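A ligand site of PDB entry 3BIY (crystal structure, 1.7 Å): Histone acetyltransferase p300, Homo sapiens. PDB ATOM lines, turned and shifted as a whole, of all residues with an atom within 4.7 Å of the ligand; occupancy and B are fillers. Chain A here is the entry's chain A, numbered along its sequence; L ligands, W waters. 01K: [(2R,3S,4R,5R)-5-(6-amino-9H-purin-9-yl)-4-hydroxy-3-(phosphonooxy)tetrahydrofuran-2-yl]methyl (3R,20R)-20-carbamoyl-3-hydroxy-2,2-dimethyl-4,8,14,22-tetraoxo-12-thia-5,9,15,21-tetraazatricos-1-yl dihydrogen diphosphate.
N of Leu 112 lies within hydrogen-bond range of O32 of the ligand (2.9 Å).
A sulfur (S20) of the ligand sits close to the backbone NH (N) of Cys 152 (3.7 Å).
NE1 of Trp 180 is in hydrogen-bond range of O36 of the ligand (2.8 Å).
N64 of the ligand lies within hydrogen-bond range of OH of Tyr 111 (3.2 Å).
NZ of the ligand sits at hydrogen-bond distance from O of Trp 150 (3.0 Å).
The side-chain hydroxyl (OH) of Tyr 181 sits close to a sulfur (S20) of the ligand, 3.1 Å away.
OG1 of Thr 125 lies within hydrogen-bond range of O36 of the ligand (2.7 Å).
The guanidinium group (NH1) of Arg 176 is in hydrogen-bond range of an oxygen (O60) of the ligand, at 3.2 Å.
A nitrogen (N59) of the ligand sits at hydrogen-bond distance from the backbone carbonyl oxygen of Ile 171, 2.9 Å away.
The backbone carbonyl oxygen of Leu 112 lies within hydrogen-bond range of a nitrogen (N17) of the ligand.
The side-chain hydroxyl of Ser 114 lies within hydrogen-bond range of an oxygen (O34) of the ligand.
The backbone NH (N) of Ser 114 sits at hydrogen-bond distance from an oxygen (O34) of the ligand, at 3.1 Å.
O35 of the ligand lies within salt-bridge range of NE of Arg 124 (2.9 Å).
The backbone carbonyl oxygen (O) of Pro 153 sits close to the side-chain hydroxyl (OH) of Tyr 160 (3.3 Å).
The backbone carbonyl oxygen of Ser 114 lies within hydrogen-bond range of the side-chain amide nitrogen of Gln 169 (3.1 Å).
The side-chain hydroxyl (OG) of Ser 114 sits close to the side-chain hydroxyl (OH) of Tyr 128, 3.3 Å away.
O of Cys 152 is in hydrogen-bond range of OH of Tyr 160, 2.7 Å away.
The backbone nitrogen (N) of Pro 172 lies close to a nitrogen (N52) of the ligand, 3.4 Å away.
Ser 110 touches the ligand.
Asp 113 touches the ligand (OD1 to C15, 3.5 Å).
Tyr 128 touches the ligand.
CA of Ala 151 touches S20 of the ligand (3.7 Å).
Pro 153 touches the ligand (CA to O33, 3.8 Å).
Pro 154 touches the ligand.
CE2 of Tyr 160 touches N17 of the ligand, 3.6 Å away.
NE2 of Gln 169 touches O34 of the ligand, 3.9 Å away.
Lys 170 touches the ligand.
CD2 of Leu 177 touches S20 of the ligand, 3.8 Å away.
Hydrophobic or aromatic side chains that line the ligand: Tyr 111, Leu 112, Tyr 128, Trp 150, Pro 154, Tyr 160, Pro 172, Leu 177, Trp 180 and Tyr 181.
Within 4 Å of the ligand: Ser 110, Tyr 111, Leu 112, Asp 113, Ser 114, Arg 124, Thr 125, Tyr 128, Trp 150, Ala 151, Cys 152, Pro 153, Pro 154, Tyr 160, Gln 169, Lys 170, Ile 171, Pro 172, Arg 176, Leu 177, Trp 180 and Tyr 181.
Along chain A the residues within 4 Å of the ligand span positions 110 to 181.
The nearest printed residue that does not touch the ligand is Lys 173 (4.1 Å).
Water W10 lies within hydrogen-bond range of O46 of the ligand (2.4 Å) and NH2 of Arg 124 (3.5 Å).
Water W11 bridges an oxygen (O44) of the ligand (2.7 Å) and the side-chain amino group (NZ) of Lys 121 (2.9 Å).
Water W16 lies within hydrogen-bond range of the side-chain amino group (NZ) of Lys 173 (2.9 Å) and a nitrogen (N59) of the ligand (3.0 Å).
Water W4 lies within hydrogen-bond range of O of Lys 170, O11 of the ligand and NE2 of Gln 169.
Water W1 bridges NH1 of Arg 124 (2.9 Å) and O44 of the ligand (3.0 Å).
Water W2 lies within hydrogen-bond range of the side-chain hydroxyl of Tyr 160 (3.0 Å), the backbone carbonyl oxygen of Pro 153 (3.1 Å), a nitrogen (N) of the ligand (3.5 Å) and the side-chain sulfur of Cys 152 (3.7 Å).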
ATOM      1  N   ILE A 109      41.130   8.078 -23.262  1.00  0.00           N
ATOM      2  CA  ILE A 109      40.012   7.433 -22.519  1.00  0.00           C
ATOM      3  C   ILE A 109      40.332   5.981 -22.146  1.00  0.00           C
ATOM      4  O   ILE A 109      40.504   5.099 -23.014  1.00  0.00           O
ATOM      5  CB  ILE A 109      38.695   7.464 -23.307  1.00  0.00           C
ATOM      6  CG1 ILE A 109      38.358   8.877 -23.784  1.00  0.00           C
ATOM      7  CG2 ILE A 109      37.545   6.814 -22.490  1.00  0.00           C
ATOM      8  CD1 ILE A 109      38.738   9.992 -22.881  1.00  0.00           C
ATOM      9  N   SER A 110      40.431   5.719 -20.842  1.00  0.00           N
ATOM     10  CA  SER A 110      40.730   4.392 -20.376  1.00  0.00           C
ATOM     11  C   SER A 110      39.511   3.479 -20.532  1.00  0.00           C
ATOM     12  O   SER A 110      39.600   2.383 -21.113  1.00  0.00           O
ATOM     13  CB  SER A 110      41.142   4.436 -18.906  1.00  0.00           C
ATOM     14  OG  SER A 110      42.396   5.085 -18.766  1.00  0.00           O
ATOM     15  N   TYR A 111      38.380   3.951 -20.015  1.00  0.00           N
ATOM     16  CA  TYR A 111      37.118   3.224 -20.031  1.00  0.00           C
ATOM     17  C   TYR A 111      35.970   4.203 -20.042  1.00  0.00           C
ATOM     18  O   TYR A 111      36.047   5.227 -19.358  1.00  0.00           O
ATOM     19  CB  TYR A 111      36.957   2.378 -18.770  1.00  0.00           C
ATOM     20  CG  TYR A 111      37.907   1.219 -18.738  1.00  0.00           C
ATOM     21  CD1 TYR A 111      37.644   0.059 -19.465  1.00  0.00           C
ATOM     22  CD2 TYR A 111      39.094   1.286 -17.999  1.00  0.00           C
ATOM     23  CE1 TYR A 111      38.532  -1.018 -19.466  1.00  0.00           C
ATOM     24  CE2 TYR A 111      39.988   0.216 -17.985  1.00  0.00           C
ATOM     25  CZ  TYR A 111      39.707  -0.931 -18.717  1.00  0.00           C
ATOM     26  OH  TYR A 111      40.593  -1.995 -18.683  1.00  0.00           O
ATOM     27  N   LEU A 112      34.909   3.848 -20.761  1.00  0.00           N
ATOM     28  CA  LEU A 112      33.684   4.623 -20.759  1.00  0.00           C
ATOM     29  C   LEU A 112      32.527   3.632 -20.669  1.00  0.00           C
ATOM     30  O   LEU A 112      32.565   2.580 -21.297  1.00  0.00           O
ATOM     31  CB  LEU A 112      33.601   5.388 -22.065  1.00  0.00           C
ATOM     32  CG  LEU A 112      32.440   6.273 -22.390  1.00  0.00           C
ATOM     33  CD1 LEU A 112      32.956   7.358 -23.323  1.00  0.00           C
ATOM     34  CD2 LEU A 112      31.337   5.467 -23.052  1.00  0.00           C
ATOM     35  N   ASP A 113      31.502   3.957 -19.879  1.00  0.00           N
ATOM     36  CA  ASP A 113      30.380   3.008 -19.755  1.00  0.00           C
ATOM     37  C   ASP A 113      29.109   3.770 -19.409  1.00  0.00           C
ATOM     38  O   ASP A 113      29.159   4.889 -18.917  1.00  0.00           O
ATOM     39  CB  ASP A 113      30.707   1.998 -18.645  1.00  0.00           C
ATOM     40  CG  ASP A 113      29.873   0.715 -18.694  1.00  0.00           C
ATOM     41  OD1 ASP A 113      29.105   0.483 -19.658  1.00  0.00           O
ATOM     42  OD2 ASP A 113      30.007  -0.117 -17.745  1.00  0.00           O
ATOM     43  N   SER A 114      27.970   3.127 -19.642  1.00  0.00           N
ATOM     44  CA  SER A 114      26.687   3.755 -19.338  1.00  0.00           C
ATOM     45  C   SER A 114      25.648   2.696 -19.055  1.00  0.00           C
ATOM     46  O   SER A 114      25.816   1.525 -19.405  1.00  0.00           O
ATOM     47  CB  SER A 114      26.227   4.565 -20.536  1.00  0.00           C
ATOM     48  OG  SER A 114      25.796   3.670 -21.585  1.00  0.00           O
ATOM     49  N   LYS A 121      14.451   9.042 -23.251  1.00  0.00           N
ATOM     50  CA  LYS A 121      15.240   8.204 -24.170  1.00  0.00           C
ATOM     51  C   LYS A 121      15.817   8.986 -25.325  1.00  0.00           C
ATOM     52  O   LYS A 121      16.973   8.742 -25.719  1.00  0.00           O
ATOM     53  CB  LYS A 121      14.369   7.068 -24.739  1.00  0.00           C
ATOM     54  CG  LYS A 121      14.234   5.900 -23.832  1.00  0.00           C
ATOM     55  CD  LYS A 121      13.219   4.930 -24.421  1.00  0.00           C
ATOM     56  CE  LYS A 121      13.855   4.058 -25.482  1.00  0.00           C
ATOM     57  NZ  LYS A 121      12.905   2.965 -25.899  1.00  0.00           N
ATOM     58  N   ARG A 124      19.255  10.672 -24.733  1.00  0.00           N
ATOM     59  CA  ARG A 124      20.347   9.934 -24.086  1.00  0.00           C
ATOM     60  C   ARG A 124      21.666  10.063 -24.855  1.00  0.00           C
ATOM     61  O   ARG A 124      22.665  10.489 -24.305  1.00  0.00           O
ATOM     62  CB  ARG A 124      19.915   8.451 -23.963  1.00  0.00           C
ATOM     63  CG  ARG A 124      20.971   7.586 -23.247  1.00  0.00           C
ATOM     64  CD  ARG A 124      20.672   6.107 -23.309  1.00  0.00           C
ATOM     65  NE  ARG A 124      20.716   5.601 -24.692  1.00  0.00           N
ATOM     66  CZ  ARG A 124      19.675   5.390 -25.462  1.00  0.00           C
ATOM     67  NH1 ARG A 124      18.418   5.588 -25.023  1.00  0.00           N
ATOM     68  NH2 ARG A 124      19.874   4.971 -26.714  1.00  0.00           N
ATOM     69  N   THR A 125      21.662   9.660 -26.138  1.00  0.00           N
ATOM     70  CA  THR A 125      22.915   9.725 -26.927  1.00  0.00           C
ATOM     71  C   THR A 125      23.421  11.149 -26.984  1.00  0.00           C
ATOM     72  O   THR A 125      24.619  11.389 -26.794  1.00  0.00           O
ATOM     73  CB  THR A 125      22.685   9.192 -28.314  1.00  0.00           C
ATOM     74  OG1 THR A 125      22.363   7.801 -28.213  1.00  0.00           O
ATOM     75  CG2 THR A 125      23.963   9.380 -29.201  1.00  0.00           C
ATOM     76  N   TYR A 128      25.253  11.966 -23.841  1.00  0.00           N
ATOM     77  CA  TYR A 128      26.605  11.323 -23.816  1.00  0.00           C
ATOM     78  C   TYR A 128      27.570  12.131 -24.661  1.00  0.00           C
ATOM     79  O   TYR A 128      28.706  12.380 -24.264  1.00  0.00           O
ATOM     80  CB  TYR A 128      26.555   9.912 -24.377  1.00  0.00           C
ATOM     81  CG  TYR A 128      25.761   8.917 -23.560  1.00  0.00           C
ATOM     82  CD1 TYR A 128      25.574   9.073 -22.189  1.00  0.00           C
ATOM     83  CD2 TYR A 128      25.229   7.797 -24.177  1.00  0.00           C
ATOM     84  CE1 TYR A 128      24.852   8.105 -21.457  1.00  0.00           C
ATOM     85  CE2 TYR A 128      24.493   6.877 -23.475  1.00  0.00           C
ATOM     86  CZ  TYR A 128      24.318   7.014 -22.113  1.00  0.00           C
ATOM     87  OH  TYR A 128      23.566   6.049 -21.439  1.00  0.00           O
ATOM     88  N   ILE A 149      41.321   7.765 -28.511  1.00  0.00           N
ATOM     89  CA  ILE A 149      40.272   6.801 -28.146  1.00  0.00           C
ATOM     90  C   ILE A 149      40.523   5.434 -28.787  1.00  0.00           C
ATOM     91  O   ILE A 149      40.740   5.343 -29.999  1.00  0.00           O
ATOM     92  CB  ILE A 149      38.884   7.305 -28.604  1.00  0.00           C
ATOM     93  CG1 ILE A 149      38.642   8.721 -28.048  1.00  0.00           C
ATOM     94  CG2 ILE A 149      37.753   6.341 -28.175  1.00  0.00           C
ATOM     95  CD1 ILE A 149      37.259   9.311 -28.331  1.00  0.00           C
ATOM     96  N   TRP A 150      40.491   4.390 -27.955  1.00  0.00           N
ATOM     97  CA  TRP A 150      40.383   2.992 -28.427  1.00  0.00           C
ATOM     98  C   TRP A 150      38.904   2.630 -28.376  1.00  0.00           C
ATOM     99  O   TRP A 150      38.351   2.427 -27.295  1.00  0.00           O
ATOM    100  CB  TRP A 150      41.203   2.077 -27.525  1.00  0.00           C
ATOM    101  CG  TRP A 150      41.227   0.603 -27.866  1.00  0.00           C
ATOM    102  CD1 TRP A 150      40.724   0.018 -29.006  1.00  0.00           C
ATOM    103  CD2 TRP A 150      41.840  -0.433 -27.113  1.00  0.00           C
ATOM    104  NE1 TRP A 150      40.932  -1.354 -28.967  1.00  0.00           N
ATOM    105  CE2 TRP A 150      41.630  -1.649 -27.828  1.00  0.00           C
ATOM    106  CE3 TRP A 150      42.516  -0.470 -25.887  1.00  0.00           C
ATOM    107  CZ2 TRP A 150      42.103  -2.874 -27.353  1.00  0.00           C
ATOM    108  CZ3 TRP A 150      42.988  -1.714 -25.416  1.00  0.00           C
ATOM    109  CH2 TRP A 150      42.773  -2.893 -26.159  1.00  0.00           C
ATOM    110  N   ALA A 151      38.248   2.601 -29.540  1.00  0.00           N
ATOM    111  CA  ALA A 151      36.791   2.357 -29.611  1.00  0.00           C
ATOM    112  C   ALA A 151      36.500   0.850 -29.598  1.00  0.00           C
ATOM    113  O   ALA A 151      36.228   0.263 -30.637  1.00  0.00           O
ATOM    114  CB  ALA A 151      36.193   3.031 -30.864  1.00  0.00           C
ATOM    115  N   CYS A 152      36.539   0.230 -28.426  1.00  0.00           N
ATOM    116  CA  CYS A 152      36.403  -1.208 -28.341  1.00  0.00           C
ATOM    117  C   CYS A 152      35.262  -1.559 -27.394  1.00  0.00           C
ATOM    118  O   CYS A 152      35.359  -1.261 -26.212  1.00  0.00           O
ATOM    119  CB  CYS A 152      37.699  -1.799 -27.797  1.00  0.00           C
ATOM    120  SG  CYS A 152      37.768  -3.590 -27.826  1.00  0.00           S
ATOM    121  N   PRO A 153      34.166  -2.140 -27.918  1.00  0.00           N
ATOM    122  CA  PRO A 153      33.118  -2.526 -26.969  1.00  0.00           C
ATOM    123  C   PRO A 153      33.512  -3.696 -26.074  1.00  0.00           C
ATOM    124  O   PRO A 153      34.410  -4.482 -26.423  1.00  0.00           O
ATOM    125  CB  PRO A 153      31.916  -2.899 -27.854  1.00  0.00           C
ATOM    126  CG  PRO A 153      32.393  -2.862 -29.281  1.00  0.00           C
ATOM    127  CD  PRO A 153      33.830  -2.459 -29.320  1.00  0.00           C
ATOM    128  N   PRO A 154      32.858  -3.821 -24.909  1.00  0.00           N
ATOM    129  CA  PRO A 154      33.164  -4.925 -24.017  1.00  0.00           C
ATOM    130  C   PRO A 154      32.807  -6.264 -24.655  1.00  0.00           C
ATOM    131  O   PRO A 154      31.893  -6.327 -25.473  1.00  0.00           O
ATOM    132  CB  PRO A 154      32.267  -4.672 -22.795  1.00  0.00           C
ATOM    133  CG  PRO A 154      31.207  -3.719 -23.262  1.00  0.00           C
ATOM    134  CD  PRO A 154      31.829  -2.910 -24.359  1.00  0.00           C
ATOM    135  N   TYR A 160      32.413  -2.823 -18.212  1.00  0.00           N
ATOM    136  CA  TYR A 160      33.582  -1.973 -18.036  1.00  0.00           C
ATOM    137  C   TYR A 160      33.577  -1.277 -16.686  1.00  0.00           C
ATOM    138  O   TYR A 160      34.578  -1.326 -15.986  1.00  0.00           O
ATOM    139  CB  TYR A 160      33.683  -0.914 -19.135  1.00  0.00           C
ATOM    140  CG  TYR A 160      34.258  -1.424 -20.428  1.00  0.00           C
ATOM    141  CD1 TYR A 160      34.944  -2.642 -20.491  1.00  0.00           C
ATOM    142  CD2 TYR A 160      34.162  -0.663 -21.574  1.00  0.00           C
ATOM    143  CE1 TYR A 160      35.495  -3.101 -21.684  1.00  0.00           C
ATOM    144  CE2 TYR A 160      34.713  -1.098 -22.785  1.00  0.00           C
ATOM    145  CZ  TYR A 160      35.383  -2.308 -22.832  1.00  0.00           C
ATOM    146  OH  TYR A 160      35.944  -2.749 -24.017  1.00  0.00           O
ATOM    147  N   GLN A 169      19.863  -3.981 -22.634  1.00  0.00           N
ATOM    148  CA  GLN A 169      20.736  -2.934 -23.149  1.00  0.00           C
ATOM    149  C   GLN A 169      21.673  -3.561 -24.172  1.00  0.00           C
ATOM    150  O   GLN A 169      22.605  -4.293 -23.795  1.00  0.00           O
ATOM    151  CB  GLN A 169      21.561  -2.282 -22.053  1.00  0.00           C
ATOM    152  CG  GLN A 169      22.384  -1.086 -22.582  1.00  0.00           C
ATOM    153  CD  GLN A 169      23.088  -0.319 -21.472  1.00  0.00           C
ATOM    154  OE1 GLN A 169      22.561  -0.181 -20.365  1.00  0.00           O
ATOM    155  NE2 GLN A 169      24.279   0.229 -21.791  1.00  0.00           N
ATOM    156  N   LYS A 170      21.437  -3.277 -25.454  1.00  0.00           N
ATOM    157  CA  LYS A 170      22.309  -3.848 -26.483  1.00  0.00           C
ATOM    158  C   LYS A 170      23.681  -3.205 -26.392  1.00  0.00           C
ATOM    159  O   LYS A 170      23.795  -1.997 -26.132  1.00  0.00           O
ATOM    160  CB  LYS A 170      21.723  -3.627 -27.866  1.00  0.00           C
ATOM    161  CG  LYS A 170      20.383  -4.308 -28.073  1.00  0.00           C
ATOM    162  CD  LYS A 170      19.910  -4.123 -29.502  1.00  0.00           C
ATOM    163  CE  LYS A 170      18.687  -4.980 -29.815  1.00  0.00           C
ATOM    164  NZ  LYS A 170      17.432  -4.286 -29.398  1.00  0.00           N
ATOM    165  N   ILE A 171      24.707  -4.024 -26.613  1.00  0.00           N
ATOM    166  CA  ILE A 171      26.090  -3.526 -26.702  1.00  0.00           C
ATOM    167  C   ILE A 171      26.443  -3.349 -28.178  1.00  0.00           C
ATOM    168  O   ILE A 171      26.289  -4.290 -28.990  1.00  0.00           O
ATOM    169  CB  ILE A 171      27.085  -4.510 -26.036  1.00  0.00           C
ATOM    170  CG1 ILE A 171      26.720  -4.735 -24.575  1.00  0.00           C
ATOM    171  CG2 ILE A 171      28.536  -3.975 -26.120  1.00  0.00           C
ATOM    172  CD1 ILE A 171      26.578  -6.171 -24.214  1.00  0.00           C
ATOM    173  N   PRO A 172      26.898  -2.158 -28.560  1.00  0.00           N
ATOM    174  CA  PRO A 172      27.198  -1.941 -29.974  1.00  0.00           C
ATOM    175  C   PRO A 172      28.350  -2.815 -30.439  1.00  0.00           C
ATOM    176  O   PRO A 172      29.250  -3.113 -29.656  1.00  0.00           O
ATOM    177  CB  PRO A 172      27.629  -0.474 -30.022  1.00  0.00           C
ATOM    178  CG  PRO A 172      27.992  -0.110 -28.643  1.00  0.00           C
ATOM    179  CD  PRO A 172      27.137  -0.967 -27.737  1.00  0.00           C
ATOM    180  N   LYS A 173      28.285  -3.243 -31.688  1.00  0.00           N
ATOM    181  CA  LYS A 173      29.434  -3.868 -32.350  1.00  0.00           C
ATOM    182  C   LYS A 173      30.422  -2.792 -32.742  1.00  0.00           C
ATOM    183  O   LYS A 173      30.080  -1.629 -32.738  1.00  0.00           O
ATOM    184  CB  LYS A 173      28.968  -4.687 -33.554  1.00  0.00           C
ATOM    185  CG  LYS A 173      28.163  -5.926 -33.159  1.00  0.00           C
ATOM    186  CD  LYS A 173      28.984  -6.939 -32.321  1.00  0.00           C
ATOM    187  CE  LYS A 173      28.314  -8.320 -32.194  1.00  0.00           C
ATOM    188  NZ  LYS A 173      27.194  -8.385 -31.201  1.00  0.00           N
ATOM    189  N   ARG A 176      29.273   0.050 -35.282  1.00  0.00           N
ATOM    190  CA  ARG A 176      28.319   0.975 -34.674  1.00  0.00           C
ATOM    191  C   ARG A 176      29.009   1.936 -33.698  1.00  0.00           C
ATOM    192  O   ARG A 176      28.730   3.149 -33.700  1.00  0.00           O
ATOM    193  CB  ARG A 176      27.219   0.155 -33.980  1.00  0.00           C
ATOM    194  CG  ARG A 176      26.194   1.054 -33.286  1.00  0.00           C
ATOM    195  CD  ARG A 176      25.071   0.250 -32.610  1.00  0.00           C
ATOM    196  NE  ARG A 176      24.247  -0.437 -33.591  1.00  0.00           N
ATOM    197  CZ  ARG A 176      23.234   0.125 -34.249  1.00  0.00           C
ATOM    198  NH1 ARG A 176      22.935   1.416 -34.045  1.00  0.00           N
ATOM    199  NH2 ARG A 176      22.559  -0.592 -35.126  1.00  0.00           N
ATOM    200  N   LEU A 177      29.917   1.414 -32.878  1.00  0.00           N
ATOM    201  CA  LEU A 177      30.606   2.241 -31.895  1.00  0.00           C
ATOM    202  C   LEU A 177      31.502   3.268 -32.604  1.00  0.00           C
ATOM    203  O   LEU A 177      31.559   4.432 -32.223  1.00  0.00           O
ATOM    204  CB  LEU A 177      31.425   1.368 -30.951  1.00  0.00           C
ATOM    205  CG  LEU A 177      32.104   2.177 -29.843  1.00  0.00           C
ATOM    206  CD1 LEU A 177      31.103   2.982 -29.002  1.00  0.00           C
ATOM    207  CD2 LEU A 177      32.890   1.174 -28.996  1.00  0.00           C
ATOM    208  N   TRP A 180      29.406   5.996 -33.874  1.00  0.00           N
ATOM    209  CA  TRP A 180      28.970   6.776 -32.721  1.00  0.00           C
ATOM    210  C   TRP A 180      30.048   7.831 -32.388  1.00  0.00           C
ATOM    211  O   TRP A 180      29.728   8.998 -32.173  1.00  0.00           O
ATOM    212  CB  TRP A 180      28.747   5.821 -31.555  1.00  0.00           C
ATOM    213  CG  TRP A 180      28.123   6.399 -30.281  1.00  0.00           C
ATOM    214  CD1 TRP A 180      26.799   6.501 -30.001  1.00  0.00           C
ATOM    215  CD2 TRP A 180      28.834   6.834 -29.111  1.00  0.00           C
ATOM    216  NE1 TRP A 180      26.637   7.011 -28.703  1.00  0.00           N
ATOM    217  CE2 TRP A 180      27.867   7.220 -28.150  1.00  0.00           C
ATOM    218  CE3 TRP A 180      30.199   6.920 -28.768  1.00  0.00           C
ATOM    219  CZ2 TRP A 180      28.219   7.708 -26.862  1.00  0.00           C
ATOM    220  CZ3 TRP A 180      30.563   7.388 -27.490  1.00  0.00           C
ATOM    221  CH2 TRP A 180      29.560   7.789 -26.542  1.00  0.00           C
ATOM    222  N   TYR A 181      31.317   7.420 -32.375  1.00  0.00           N
ATOM    223  CA  TYR A 181      32.394   8.376 -32.151  1.00  0.00           C
ATOM    224  C   TYR A 181      32.520   9.397 -33.270  1.00  0.00           C
ATOM    225  O   TYR A 181      32.756  10.586 -32.993  1.00  0.00           O
ATOM    226  CB  TYR A 181      33.715   7.663 -31.943  1.00  0.00           C
ATOM    227  CG  TYR A 181      33.840   7.172 -30.541  1.00  0.00           C
ATOM    228  CD1 TYR A 181      33.950   8.069 -29.478  1.00  0.00           C
ATOM    229  CD2 TYR A 181      33.862   5.826 -30.256  1.00  0.00           C
ATOM    230  CE1 TYR A 181      34.066   7.631 -28.170  1.00  0.00           C
ATOM    231  CE2 TYR A 181      34.005   5.364 -28.940  1.00  0.00           C
ATOM    232  CZ  TYR A 181      34.108   6.260 -27.914  1.00  0.00           C
ATOM    233  OH  TYR A 181      34.235   5.839 -26.598  1.00  0.00           O
HETATM  234  O1  01K L   1      24.906   2.616 -29.974  1.00  0.00           O
HETATM  235  P2  01K L   1      24.235   2.789 -28.668  1.00  0.00           P
HETATM  236  O3  01K L   1      24.407   4.349 -28.246  1.00  0.00           O
HETATM  237  P4  01K L   1      24.192   5.051 -26.833  1.00  0.00           P
HETATM  238  O5  01K L   1      25.296   4.473 -25.848  1.00  0.00           O
HETATM  239  C6  01K L   1      26.657   4.378 -26.265  1.00  0.00           C
HETATM  240  C7  01K L   1      27.525   3.747 -25.174  1.00  0.00           C
HETATM  241  C8  01K L   1      28.914   3.529 -25.781  1.00  0.00           C
HETATM  242  C9  01K L   1      27.600   4.720 -23.978  1.00  0.00           C
HETATM  243  C10 01K L   1      26.849   2.419 -24.727  1.00  0.00           C
HETATM  244  O11 01K L   1      26.656   1.538 -25.846  1.00  0.00           O
HETATM  245  C12 01K L   1      27.645   1.673 -23.658  1.00  0.00           C
HETATM  246  N13 01K L   1      28.293   0.594 -24.109  1.00  0.00           N
HETATM  247  C14 01K L   1      29.068  -0.304 -23.224  1.00  0.00           C
HETATM  248  C15 01K L   1      30.416   0.324 -22.924  1.00  0.00           C
HETATM  249  C16 01K L   1      31.260   0.575 -24.190  1.00  0.00           C
HETATM  250  N17 01K L   1      32.312   1.319 -23.975  1.00  0.00           N
HETATM  251  C18 01K L   1      33.268   1.538 -25.075  1.00  0.00           C
HETATM  252  C19 01K L   1      33.615   2.942 -25.285  1.00  0.00           C
HETATM  253  S20 01K L   1      35.093   2.862 -26.348  1.00  0.00           S
HETATM  254  C21 01K L   1      36.209   3.645 -25.119  1.00  0.00           C
HETATM  255  C22 01K L   1      36.613   2.582 -24.108  1.00  0.00           C
HETATM  256  NZ  01K L   1      37.640   1.829 -24.493  1.00  0.00           N
HETATM  257  CE  01K L   1      38.112   0.763 -23.620  1.00  0.00           C
HETATM  258  CD  01K L   1      38.992  -0.173 -24.397  1.00  0.00           C
HETATM  259  CG  01K L   1      39.314  -1.353 -23.490  1.00  0.00           C
HETATM  260  CB  01K L   1      39.981  -2.435 -24.301  1.00  0.00           C
HETATM  261  CA  01K L   1      39.593  -3.828 -23.808  1.00  0.00           C
HETATM  262  N   01K L   1      40.267  -4.898 -24.580  1.00  0.00           N
HETATM  263  C   01K L   1      39.643  -3.996 -22.274  1.00  0.00           C
HETATM  264  O   01K L   1      38.810  -4.710 -21.741  1.00  0.00           O
HETATM  265  O33 01K L   1      31.005   0.083 -25.291  1.00  0.00           O
HETATM  266  O34 01K L   1      27.649   2.050 -22.490  1.00  0.00           O
HETATM  267  O35 01K L   1      22.886   4.587 -26.314  1.00  0.00           O
HETATM  268  O36 01K L   1      24.400   6.487 -27.064  1.00  0.00           O
HETATM  269  O37 01K L   1      24.606   1.879 -27.552  1.00  0.00           O
HETATM  270  O38 01K L   1      22.695   2.679 -28.861  1.00  0.00           O
HETATM  271  C40 01K L   1      20.901   2.575 -30.465  1.00  0.00           C
HETATM  272  C41 01K L   1      19.951   1.980 -29.427  1.00  0.00           C
HETATM  273  O45 01K L   1      16.460   2.872 -30.816  1.00  0.00           O
HETATM  274  O46 01K L   1      18.272   4.481 -29.857  1.00  0.00           O
HETATM  275  C54 01K L   1      22.046  -1.873 -31.318  1.00  0.00           C
HETATM  276  C63 01K L   1      42.109  -5.458 -22.998  1.00  0.00           C
HETATM  277  C61 01K L   1      41.332  -5.658 -24.295  1.00  0.00           C
HETATM  278  O62 01K L   1      41.711  -6.517 -25.077  1.00  0.00           O
HETATM  279  N64 01K L   1      40.589  -3.358 -21.604  1.00  0.00           N
HETATM  280  O32 01K L   1      36.001   2.418 -23.055  1.00  0.00           O
HETATM  281  C39 01K L   1      21.989   3.457 -29.818  1.00  0.00           C
HETATM  282  O60 01K L   1      21.597   1.495 -31.108  1.00  0.00           O
HETATM  283  O42 01K L   1      18.649   1.883 -30.056  1.00  0.00           O
HETATM  284  P43 01K L   1      17.646   3.120 -29.829  1.00  0.00           P
HETATM  285  O44 01K L   1      17.109   2.697 -28.361  1.00  0.00           O
HETATM  286  C47 01K L   1      20.523   0.584 -29.220  1.00  0.00           C
HETATM  287  O48 01K L   1      19.474  -0.336 -28.868  1.00  0.00           O
HETATM  288  C49 01K L   1      21.001   0.276 -30.660  1.00  0.00           C
HETATM  289  N50 01K L   1      22.052  -0.763 -30.592  1.00  0.00           N
HETATM  290  C51 01K L   1      23.145  -0.772 -29.810  1.00  0.00           C
HETATM  291  N52 01K L   1      23.829  -1.915 -30.026  1.00  0.00           N
HETATM  292  C53 01K L   1      23.165  -2.603 -30.947  1.00  0.00           C
HETATM  293  N55 01K L   1      21.166  -2.358 -32.228  1.00  0.00           N
HETATM  294  C56 01K L   1      21.423  -3.536 -32.795  1.00  0.00           C
HETATM  295  N57 01K L   1      22.509  -4.264 -32.471  1.00  0.00           N
HETATM  296  C58 01K L   1      23.387  -3.833 -31.551  1.00  0.00           C
HETATM  297  N59 01K L   1      24.450  -4.569 -31.228  1.00  0.00           N
HETATM  298  O   HOH W   1      16.451   5.391 -27.189  1.00  0.00           O
HETATM  299  O   HOH W   2      36.854  -5.474 -24.728  1.00  0.00           O
HETATM  300  O   HOH W   3      22.628   0.395 -26.358  1.00  0.00           O
HETATM  301  O   HOH W   4      25.476  -0.768 -24.352  1.00  0.00           O
HETATM  302  O   HOH W   5      18.925  -1.323 -33.557  1.00  0.00           O
HETATM  303  O   HOH W   6      27.768   2.995 -29.931  1.00  0.00           O
HETATM  304  O   HOH W   7      22.397   2.508 -24.646  1.00  0.00           O
HETATM  305  O   HOH W   8      24.386   3.721 -32.350  1.00  0.00           O
HETATM  306  O   HOH W   9      39.573   4.367 -25.252  1.00  0.00           O
HETATM  307  O   HOH W  10      18.946   6.791 -29.551  1.00  0.00           O
HETATM  308  O   HOH W  11      14.532   1.887 -27.997  1.00  0.00           O
HETATM  309  O   HOH W  12      25.970  -2.928 -33.684  1.00  0.00           O
HETATM  310  O   HOH W  13      42.527  -1.272 -21.340  1.00  0.00           O
HETATM  311  O   HOH W  14      19.629  -1.339 -26.366  1.00  0.00           O
HETATM  312  O   HOH W  15      24.921  -5.230 -34.688  1.00  0.00           O
HETATM  313  O   HOH W  16      24.678  -7.381 -32.192  1.00  0.00           O
